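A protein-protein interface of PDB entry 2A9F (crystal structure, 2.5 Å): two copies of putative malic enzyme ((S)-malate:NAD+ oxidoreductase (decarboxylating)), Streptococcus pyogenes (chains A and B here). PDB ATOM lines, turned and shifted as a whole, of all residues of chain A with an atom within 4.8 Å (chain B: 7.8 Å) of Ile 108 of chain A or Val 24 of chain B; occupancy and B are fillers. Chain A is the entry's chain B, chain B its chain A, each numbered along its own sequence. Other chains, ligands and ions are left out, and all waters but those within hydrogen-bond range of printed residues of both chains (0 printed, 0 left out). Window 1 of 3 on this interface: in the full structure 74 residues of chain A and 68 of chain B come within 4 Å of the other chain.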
ATOM      1  N   LEU A  22      -9.630  -9.554 -13.955  1.00  0.00           N
ATOM      2  CA  LEU A  22      -8.520  -8.739 -13.443  1.00  0.00           C
ATOM      3  C   LEU A  22      -7.500  -8.324 -14.488  1.00  0.00           C
ATOM      4  O   LEU A  22      -7.418  -8.900 -15.564  1.00  0.00           O
ATOM      5  CB  LEU A  22      -7.746  -9.499 -12.372  1.00  0.00           C
ATOM      6  CG  LEU A  22      -8.468 -10.200 -11.237  1.00  0.00           C
ATOM      7  CD1 LEU A  22      -7.411 -10.916 -10.419  1.00  0.00           C
ATOM      8  CD2 LEU A  22      -9.266  -9.209 -10.385  1.00  0.00           C
ATOM      9  N   GLU A  23      -6.703  -7.330 -14.123  1.00  0.00           N
ATOM     10  CA  GLU A  23      -5.641  -6.830 -14.973  1.00  0.00           C
ATOM     11  C   GLU A  23      -4.598  -6.152 -14.081  1.00  0.00           C
ATOM     12  O   GLU A  23      -4.915  -5.699 -12.980  1.00  0.00           O
ATOM     13  CB  GLU A  23      -6.185  -5.848 -16.017  1.00  0.00           C
ATOM     14  CG  GLU A  23      -6.496  -4.464 -15.511  1.00  0.00           C
ATOM     15  CD  GLU A  23      -6.765  -3.501 -16.650  1.00  0.00           C
ATOM     16  OE1 GLU A  23      -5.955  -3.465 -17.604  1.00  0.00           O
ATOM     17  OE2 GLU A  23      -7.779  -2.770 -16.596  1.00  0.00           O
ATOM     18  N   VAL A  24      -3.353  -6.112 -14.550  1.00  0.00           N
ATOM     19  CA  VAL A  24      -2.242  -5.503 -13.816  1.00  0.00           C
ATOM     20  C   VAL A  24      -1.979  -4.084 -14.322  1.00  0.00           C
ATOM     21  O   VAL A  24      -1.848  -3.868 -15.519  1.00  0.00           O
ATOM     22  CB  VAL A  24      -0.950  -6.345 -13.981  1.00  0.00           C
ATOM     23  CG1 VAL A  24       0.205  -5.654 -13.311  1.00  0.00           C
ATOM     24  CG2 VAL A  24      -1.148  -7.720 -13.387  1.00  0.00           C
ATOM     25  N   THR A  67       0.180  -6.959  -1.660  1.00  0.00           N
ATOM     26  CA  THR A  67      -0.381  -8.026  -2.477  1.00  0.00           C
ATOM     27  C   THR A  67      -0.499  -9.394  -1.812  1.00  0.00           C
ATOM     28  O   THR A  67       0.488  -9.994  -1.392  1.00  0.00           O
ATOM     29  CB  THR A  67       0.409  -8.211  -3.781  1.00  0.00           C
ATOM     30  OG1 THR A  67       1.774  -8.503  -3.467  1.00  0.00           O
ATOM     31  CG2 THR A  67       0.351  -6.962  -4.633  1.00  0.00           C
ATOM     32  N   VAL A  68      -1.729  -9.881  -1.724  1.00  0.00           N
ATOM     33  CA  VAL A  68      -1.999 -11.187  -1.161  1.00  0.00           C
ATOM     34  C   VAL A  68      -2.427 -12.111  -2.297  1.00  0.00           C
ATOM     35  O   VAL A  68      -3.097 -11.688  -3.224  1.00  0.00           O
ATOM     36  CB  VAL A  68      -3.118 -11.133  -0.134  1.00  0.00           C
ATOM     37  CG1 VAL A  68      -3.444 -12.538   0.314  1.00  0.00           C
ATOM     38  CG2 VAL A  68      -2.699 -10.268   1.052  1.00  0.00           C
ATOM     39  N   ALA A  69      -2.034 -13.375  -2.226  1.00  0.00           N
ATOM     40  CA  ALA A  69      -2.383 -14.321  -3.274  1.00  0.00           C
ATOM     41  C   ALA A  69      -3.523 -15.240  -2.868  1.00  0.00           C
ATOM     42  O   ALA A  69      -3.548 -15.765  -1.754  1.00  0.00           O
ATOM     43  CB  ALA A  69      -1.156 -15.153  -3.662  1.00  0.00           C
ATOM     44  N   VAL A  70      -4.473 -15.420  -3.778  1.00  0.00           N
ATOM     45  CA  VAL A  70      -5.603 -16.290  -3.533  1.00  0.00           C
ATOM     46  C   VAL A  70      -5.256 -17.603  -4.200  1.00  0.00           C
ATOM     47  O   VAL A  70      -5.389 -17.745  -5.411  1.00  0.00           O
ATOM     48  CB  VAL A  70      -6.873 -15.716  -4.158  1.00  0.00           C
ATOM     49  CG1 VAL A  70      -8.049 -16.625  -3.841  1.00  0.00           C
ATOM     50  CG2 VAL A  70      -7.104 -14.280  -3.642  1.00  0.00           C
ATOM     51  N   ALA A  96     -10.250 -12.441  -5.654  1.00  0.00           N
ATOM     52  CA  ALA A  96      -9.175 -11.446  -5.685  1.00  0.00           C
ATOM     53  C   ALA A  96      -9.743 -10.042  -5.917  1.00  0.00           C
ATOM     54  O   ALA A  96      -9.308  -9.066  -5.289  1.00  0.00           O
ATOM     55  CB  ALA A  96      -8.150 -11.793  -6.783  1.00  0.00           C
ATOM     56  N   LYS A 100      -9.660  -6.129  -3.487  1.00  0.00           N
ATOM     57  CA  LYS A 100      -9.395  -4.783  -3.951  1.00  0.00           C
ATOM     58  C   LYS A 100     -10.610  -3.897  -3.794  1.00  0.00           C
ATOM     59  O   LYS A 100     -10.495  -2.727  -3.434  1.00  0.00           O
ATOM     60  CB  LYS A 100      -8.965  -4.809  -5.419  1.00  0.00           C
ATOM     61  CG  LYS A 100      -7.696  -4.009  -5.706  1.00  0.00           C
ATOM     62  CD  LYS A 100      -7.940  -2.512  -5.626  1.00  0.00           C
ATOM     63  CE  LYS A 100      -6.662  -1.739  -5.288  1.00  0.00           C
ATOM     64  NZ  LYS A 100      -5.559  -1.979  -6.258  1.00  0.00           N
ATOM     65  N   ASP A 106      -4.365  -5.663  -2.728  1.00  0.00           N
ATOM     66  CA  ASP A 106      -4.140  -6.090  -4.104  1.00  0.00           C
ATOM     67  C   ASP A 106      -4.058  -7.611  -3.999  1.00  0.00           C
ATOM     68  O   ASP A 106      -3.351  -8.130  -3.141  1.00  0.00           O
ATOM     69  CB  ASP A 106      -2.803  -5.539  -4.646  1.00  0.00           C
ATOM     70  CG  ASP A 106      -2.886  -4.070  -5.067  1.00  0.00           C
ATOM     71  OD1 ASP A 106      -3.619  -3.751  -6.028  1.00  0.00           O
ATOM     72  OD2 ASP A 106      -2.211  -3.222  -4.438  1.00  0.00           O
ATOM     73  N   ALA A 107      -4.769  -8.331  -4.857  1.00  0.00           N
ATOM     74  CA  ALA A 107      -4.726  -9.783  -4.789  1.00  0.00           C
ATOM     75  C   ALA A 107      -4.458 -10.435  -6.135  1.00  0.00           C
ATOM     76  O   ALA A 107      -4.942  -9.965  -7.167  1.00  0.00           O
ATOM     77  CB  ALA A 107      -6.030 -10.304  -4.217  1.00  0.00           C
ATOM     78  N   ILE A 108      -3.687 -11.518  -6.130  1.00  0.00           N
ATOM     79  CA  ILE A 108      -3.410 -12.219  -7.371  1.00  0.00           C
ATOM     80  C   ILE A 108      -3.914 -13.646  -7.307  1.00  0.00           C
ATOM     81  O   ILE A 108      -3.569 -14.384  -6.398  1.00  0.00           O
ATOM     82  CB  ILE A 108      -1.890 -12.265  -7.725  1.00  0.00           C
ATOM     83  CG1 ILE A 108      -1.365 -10.860  -8.041  1.00  0.00           C
ATOM     84  CG2 ILE A 108      -1.677 -13.159  -8.946  1.00  0.00           C
ATOM     85  CD1 ILE A 108      -1.217  -9.967  -6.836  1.00  0.00           C
ATOM     86  N   PRO A 109      -4.745 -14.052  -8.279  1.00  0.00           N
ATOM     87  CA  PRO A 109      -5.279 -15.414  -8.309  1.00  0.00           C
ATOM     88  C   PRO A 109      -4.200 -16.356  -8.826  1.00  0.00           C
ATOM     89  O   PRO A 109      -3.521 -16.045  -9.802  1.00  0.00           O
ATOM     90  CB  PRO A 109      -6.436 -15.301  -9.283  1.00  0.00           C
ATOM     91  CG  PRO A 109      -5.903 -14.321 -10.291  1.00  0.00           C
ATOM     92  CD  PRO A 109      -5.277 -13.258  -9.404  1.00  0.00           C
ATOM     93  N   ILE A 110      -4.045 -17.504  -8.174  1.00  0.00           N
ATOM     94  CA  ILE A 110      -3.055 -18.490  -8.589  1.00  0.00           C
ATOM     95  C   ILE A 110      -3.571 -19.911  -8.413  1.00  0.00           C
ATOM     96  O   ILE A 110      -3.875 -20.336  -7.301  1.00  0.00           O
ATOM     97  CB  ILE A 110      -1.770 -18.344  -7.776  1.00  0.00           C
ATOM     98  CG1 ILE A 110      -0.972 -17.143  -8.276  1.00  0.00           C
ATOM     99  CG2 ILE A 110      -0.960 -19.615  -7.853  1.00  0.00           C
ATOM    100  CD1 ILE A 110       0.345 -16.993  -7.585  1.00  0.00           C
ATOM    101  N   PHE A 131       4.574 -12.247  -1.690  1.00  0.00           N
ATOM    102  CA  PHE A 131       3.346 -11.661  -1.178  1.00  0.00           C
ATOM    103  C   PHE A 131       3.495 -11.368   0.306  1.00  0.00           C
ATOM    104  O   PHE A 131       4.466 -11.797   0.950  1.00  0.00           O
ATOM    105  CB  PHE A 131       2.171 -12.608  -1.416  1.00  0.00           C
ATOM    106  CG  PHE A 131       1.901 -12.878  -2.864  1.00  0.00           C
ATOM    107  CD1 PHE A 131       2.509 -13.944  -3.506  1.00  0.00           C
ATOM    108  CD2 PHE A 131       1.043 -12.065  -3.581  1.00  0.00           C
ATOM    109  CE1 PHE A 131       2.264 -14.195  -4.843  1.00  0.00           C
ATOM    110  CE2 PHE A 131       0.793 -12.309  -4.919  1.00  0.00           C
ATOM    111  CZ  PHE A 131       1.403 -13.376  -5.550  1.00  0.00           C
ATOM    112  N   LEU B  22       3.476  -2.057  -9.070  1.00  0.00           N
ATOM    113  CA  LEU B  22       2.333  -2.685  -9.722  1.00  0.00           C
ATOM    114  C   LEU B  22       1.089  -2.639  -8.854  1.00  0.00           C
ATOM    115  O   LEU B  22       1.172  -2.447  -7.652  1.00  0.00           O
ATOM    116  CB  LEU B  22       2.641  -4.135 -10.105  1.00  0.00           C
ATOM    117  CG  LEU B  22       3.722  -4.314 -11.177  1.00  0.00           C
ATOM    118  CD1 LEU B  22       3.754  -5.769 -11.621  1.00  0.00           C
ATOM    119  CD2 LEU B  22       3.433  -3.416 -12.370  1.00  0.00           C
ATOM    120  N   GLU B  23      -0.063  -2.833  -9.484  1.00  0.00           N
ATOM    121  CA  GLU B  23      -1.354  -2.784  -8.808  1.00  0.00           C
ATOM    122  C   GLU B  23      -2.312  -3.702  -9.579  1.00  0.00           C
ATOM    123  O   GLU B  23      -2.129  -3.931 -10.776  1.00  0.00           O
ATOM    124  CB  GLU B  23      -1.842  -1.328  -8.845  1.00  0.00           C
ATOM    125  CG  GLU B  23      -3.125  -1.003  -8.121  1.00  0.00           C
ATOM    126  CD  GLU B  23      -3.473   0.481  -8.208  1.00  0.00           C
ATOM    127  OE1 GLU B  23      -4.465   0.914  -7.587  1.00  0.00           O
ATOM    128  OE2 GLU B  23      -2.756   1.221  -8.906  1.00  0.00           O
ATOM    129  N   VAL B  24      -3.311  -4.249  -8.897  1.00  0.00           N
ATOM    130  CA  VAL B  24      -4.287  -5.108  -9.564  1.00  0.00           C
ATOM    131  C   VAL B  24      -5.641  -4.406  -9.623  1.00  0.00           C
ATOM    132  O   VAL B  24      -6.227  -4.076  -8.594  1.00  0.00           O
ATOM    133  CB  VAL B  24      -4.473  -6.454  -8.847  1.00  0.00           C
ATOM    134  CG1 VAL B  24      -5.557  -7.292  -9.588  1.00  0.00           C
ATOM    135  CG2 VAL B  24      -3.140  -7.208  -8.812  1.00  0.00           C
ATOM    136  N   GLN B  25      -6.129  -4.173 -10.835  1.00  0.00           N
ATOM    137  CA  GLN B  25      -7.398  -3.497 -11.019  1.00  0.00           C
ATOM    138  C   GLN B  25      -8.421  -4.399 -11.670  1.00  0.00           C
ATOM    139  O   GLN B  25      -8.128  -5.114 -12.621  1.00  0.00           O
ATOM    140  CB  GLN B  25      -7.206  -2.256 -11.876  1.00  0.00           C
ATOM    141  CG  GLN B  25      -6.218  -1.273 -11.301  1.00  0.00           C
ATOM    142  CD  GLN B  25      -6.768  -0.519 -10.101  1.00  0.00           C
ATOM    143  OE1 GLN B  25      -7.302  -1.111  -9.153  1.00  0.00           O
ATOM    144  NE2 GLN B  25      -6.621   0.802 -10.128  1.00  0.00           N
ATOM    145  N   PRO B  26      -9.642  -4.407 -11.137  1.00  0.00           N
ATOM    146  CA  PRO B  26     -10.671  -5.260 -11.743  1.00  0.00           C
ATOM    147  C   PRO B  26     -11.110  -4.513 -12.987  1.00  0.00           C
ATOM    148  O   PRO B  26     -11.118  -3.290 -12.989  1.00  0.00           O
ATOM    149  CB  PRO B  26     -11.759  -5.297 -10.675  1.00  0.00           C
ATOM    150  CG  PRO B  26     -10.976  -5.063  -9.377  1.00  0.00           C
ATOM    151  CD  PRO B  26     -10.051  -3.950  -9.797  1.00  0.00           C
ATOM    152  N   LYS B  27     -11.432  -5.223 -14.059  1.00  0.00           N
ATOM    153  CA  LYS B  27     -11.857  -4.548 -15.276  1.00  0.00           C
ATOM    154  C   LYS B  27     -13.333  -4.785 -15.498  1.00  0.00           C
ATOM    155  O   LYS B  27     -13.876  -4.507 -16.566  1.00  0.00           O
ATOM    156  CB  LYS B  27     -11.041  -5.025 -16.484  1.00  0.00           C
ATOM    157  CG  LYS B  27     -10.888  -6.528 -16.670  1.00  0.00           C
ATOM    158  CD  LYS B  27      -9.833  -6.799 -17.753  1.00  0.00           C
ATOM    159  CE  LYS B  27      -9.592  -8.285 -17.980  1.00  0.00           C
ATOM    160  NZ  LYS B  27      -8.693  -8.523 -19.155  1.00  0.00           N
ATOM    161  N   THR B  63      -8.039 -14.827 -16.930  1.00  0.00           N
ATOM    162  CA  THR B  63      -6.944 -13.940 -17.272  1.00  0.00           C
ATOM    163  C   THR B  63      -5.753 -14.668 -17.856  1.00  0.00           C
ATOM    164  O   THR B  63      -4.778 -14.046 -18.226  1.00  0.00           O
ATOM    165  CB  THR B  63      -6.485 -13.085 -16.078  1.00  0.00           C
ATOM    166  OG1 THR B  63      -6.162 -13.923 -14.963  1.00  0.00           O
ATOM    167  CG2 THR B  63      -7.564 -12.105 -15.705  1.00  0.00           C
ATOM    168  N   THR B  67      -2.232 -12.834 -19.338  1.00  0.00           N
ATOM    169  CA  THR B  67      -1.274 -12.690 -18.248  1.00  0.00           C
ATOM    170  C   THR B  67      -0.097 -13.649 -18.264  1.00  0.00           C
ATOM    171  O   THR B  67      -0.237 -14.859 -18.364  1.00  0.00           O
ATOM    172  CB  THR B  67      -1.935 -12.791 -16.846  1.00  0.00           C
ATOM    173  OG1 THR B  67      -2.105 -14.168 -16.502  1.00  0.00           O
ATOM    174  CG2 THR B  67      -3.285 -12.076 -16.823  1.00  0.00           C
ATOM    175  N   ALA B 107       1.493  -8.835 -16.709  1.00  0.00           N
ATOM    176  CA  ALA B 107       2.569  -9.650 -16.165  1.00  0.00           C
ATOM    177  C   ALA B 107       2.602  -9.536 -14.640  1.00  0.00           C
ATOM    178  O   ALA B 107       2.559  -8.438 -14.091  1.00  0.00           O
ATOM    179  CB  ALA B 107       3.924  -9.212 -16.771  1.00  0.00           C
ATOM    180  N   ILE B 108       2.677 -10.687 -13.980  1.00  0.00           N
ATOM    181  CA  ILE B 108       2.720 -10.799 -12.528  1.00  0.00           C
ATOM    182  C   ILE B 108       4.160 -11.118 -12.114  1.00  0.00           C
ATOM    183  O   ILE B 108       4.713 -12.122 -12.531  1.00  0.00           O
ATOM    184  CB  ILE B 108       1.831 -11.992 -12.017  1.00  0.00           C
ATOM    185  CG1 ILE B 108       0.413 -11.900 -12.561  1.00  0.00           C
ATOM    186  CG2 ILE B 108       1.803 -12.010 -10.492  1.00  0.00           C
ATOM    187  CD1 ILE B 108      -0.368 -10.725 -12.058  1.00  0.00           C
ATOM    188  N   PRO B 109       4.793 -10.271 -11.295  1.00  0.00           N
ATOM    189  CA  PRO B 109       6.169 -10.609 -10.904  1.00  0.00           C
ATOM    190  C   PRO B 109       6.142 -11.657  -9.780  1.00  0.00           C
ATOM    191  O   PRO B 109       5.358 -11.536  -8.839  1.00  0.00           O
ATOM    192  CB  PRO B 109       6.733  -9.266 -10.458  1.00  0.00           C
ATOM    193  CG  PRO B 109       5.549  -8.588  -9.893  1.00  0.00           C
ATOM    194  CD  PRO B 109       4.438  -8.913 -10.857  1.00  0.00           C
ATOM    195  N   ILE B 110       6.973 -12.693  -9.887  1.00  0.00           N
ATOM    196  CA  ILE B 110       7.001 -13.759  -8.884  1.00  0.00           C
ATOM    197  C   ILE B 110       8.402 -14.267  -8.567  1.00  0.00           C
ATOM    198  O   ILE B 110       9.116 -14.767  -9.450  1.00  0.00           O
ATOM    199  CB  ILE B 110       6.147 -14.967  -9.322  1.00  0.00           C
ATOM    200  CG1 ILE B 110       4.677 -14.596  -9.268  1.00  0.00           C
ATOM    201  CG2 ILE B 110       6.390 -16.144  -8.406  1.00  0.00           C
ATOM    202  CD1 ILE B 110       3.758 -15.690  -9.763  1.00  0.00           C
ATOM    203  N   THR B 130      -2.340 -21.361 -14.296  1.00  0.00           N
ATOM    204  CA  THR B 130      -2.694 -19.978 -14.027  1.00  0.00           C
ATOM    205  C   THR B 130      -2.406 -19.005 -15.150  1.00  0.00           C
ATOM    206  O   THR B 130      -3.223 -18.127 -15.469  1.00  0.00           O
ATOM    207  CB  THR B 130      -1.923 -19.460 -12.784  1.00  0.00           C
ATOM    208  OG1 THR B 130      -2.442 -20.074 -11.597  1.00  0.00           O
ATOM    209  CG2 THR B 130      -2.036 -17.950 -12.665  1.00  0.00           C
ATOM    210  N   PHE B 131      -1.233 -19.164 -15.742  1.00  0.00           N
ATOM    211  CA  PHE B 131      -0.782 -18.248 -16.754  1.00  0.00           C
ATOM    212  C   PHE B 131      -0.868 -18.658 -18.204  1.00  0.00           C
ATOM    213  O   PHE B 131      -1.103 -19.824 -18.529  1.00  0.00           O
ATOM    214  CB  PHE B 131       0.635 -17.850 -16.395  1.00  0.00           C
ATOM    215  CG  PHE B 131       0.747 -17.295 -15.015  1.00  0.00           C
ATOM    216  CD1 PHE B 131       0.414 -15.976 -14.755  1.00  0.00           C
ATOM    217  CD2 PHE B 131       1.146 -18.108 -13.955  1.00  0.00           C
ATOM    218  CE1 PHE B 131       0.478 -15.467 -13.461  1.00  0.00           C
ATOM    219  CE2 PHE B 131       1.212 -17.610 -12.655  1.00  0.00           C
ATOM    220  CZ  PHE B 131       0.878 -16.287 -12.405  1.00  0.00           C
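Ile 108 of chain A touches just these residues of chain B: Val 24 and Ile 108.
Of chain A, only Glu 23, Lys 100, Asp 106, Ala 107 and Ile 108 come within 4 Å of Val 24 of chain B.
Ala 107 of chain A touches one residue of chain B.
Of the printed residues of chain B, Pro 109 of chain A touches Thr 130 (3.7 Å).
Of the printed residues of chain A, Ile 108 of chain B touches Val 24 (3.4 Å) and Ile 108 (3.98 Å).
Printed residues of chain A within 4 Å of Leu 22 of chain B: Val 24 (3.9 Å).
The nearest residue of chain B that does not touch Ile 108 of chain A is Phe 131 of chain B (5.3 Å).
The nearest printed residue of chain A that does not touch Thr 63 of chain B is Pro 109 of chain A (4.7 Å).
Glu 23 of chain A touches its own counterpart, Glu 23 of chain B.
Glu 23 of chain A touches Val 24 of chain B, and with the chains exchanged Val 24 of chain A touches Glu 23 of chain B.
Val 24 of chain A touches Leu 22 of chain B, but with the chains exchanged Leu 22 of chain A does not touch Val 24 of chain B (4.2 Å).
Val 24 of chain A touches Ala 107 of chain B, and with the chains exchanged Ala 107 of chain A touches Val 24 of chain B.
Of the 15 printed residues of chain A, 9 touch a printed residue of chain B.
Along chain A the printed residues that touch a printed residue of chain B span positions 22 to 110.
Of the 14 printed residues of chain B, 9 touch a printed residue of chain A.
Among the printed residues, 21 pairs touch across the chains.
NE2 of Gln 25 of chain B sits at hydrogen-bond distance from OE1 of Glu 23 of chain B (3.3 Å).
The backbone carbonyl oxygen of Thr 63 of chain B sits close to the side-chain hydroxyl of Thr 67 of chain B, at 3.2 Å.
The backbone NH of Val 68 of chain A sits at hydrogen-bond distance from the backbone carbonyl oxygen of Asp 106 of chain A (2.8 Å).
The backbone carbonyl oxygen of Val 68 of chain A is in hydrogen-bond range of the backbone NH of Ile 108 of chain A.
N of Val 70 of chain A sits at hydrogen-bond distance from O of Ile 108 of chain A (3.0 Å).
The side-chain amino group (NZ) of Lys 100 of chain A is in salt-bridge range of the side-chain carboxylate (OD1) of Asp 106 of chain A.
Among the printed residues, pairs that only touch across the chains: Leu 22 of chain A with Gln 25 of chain B (3.7 Å), Leu 22 of chain A with Lys 27 of chain B (3.3 Å), Leu 22 of chain A with Thr 63 of chain B (3.2 Å), Glu 23 of chain A with Glu 23 of chain B (3.97 Å), Glu 23 of chain A with Val 24 of chain B (3.5 Å), Glu 23 of chain A with Lys 27 of chain B (3.97 Å), Val 24 of chain A with Leu 22 of chain B (3.9 Å), Val 24 of chain A with Glu 23 of chain B (3.4 Å), Val 24 of chain A with Ala 107 of chain B (3.7 Å), Val 24 of chain A with Ile 108 of chain B (3.4 Å), Asp 106 of chain A with Glu 23 of chain B (3.5 Å), Ala 107 of chain A with Val 24 of chain B (3.7 Å), Ile 108 of chain A with Val 24 of chain B (3.9 Å), Ile 108 of chain A with Ile 108 of chain B (3.98 Å), Pro 109 of chain A with Thr 130 of chain B (3.7 Å) and Ile 110 of chain A with Thr 130 of chain B (3.4 Å).
The side-chain carboxylate (OE1) of Glu 23 of chain B is in salt-bridge range of the side-chain amino group (NZ) of Lys 100 of chain A, at 3.4 Å.
O of Val 24 of chain B sits at hydrogen-bond distance from NZ of Lys 100 of chain A (3.2 Å).
OD1 of Asp 106 of chain A is in hydrogen-bond range of N of Val 24 of chain B (2.9 Å).
The backbone NH of Gln 25 of chain B sits at hydrogen-bond distance from the backbone carbonyl oxygen of Glu 23 of chain A (2.9 Å).
NZ of Lys 100 of chain A is in hydrogen-bond range of OE1 of Gln 25 of chain B, at 3.5 Å.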
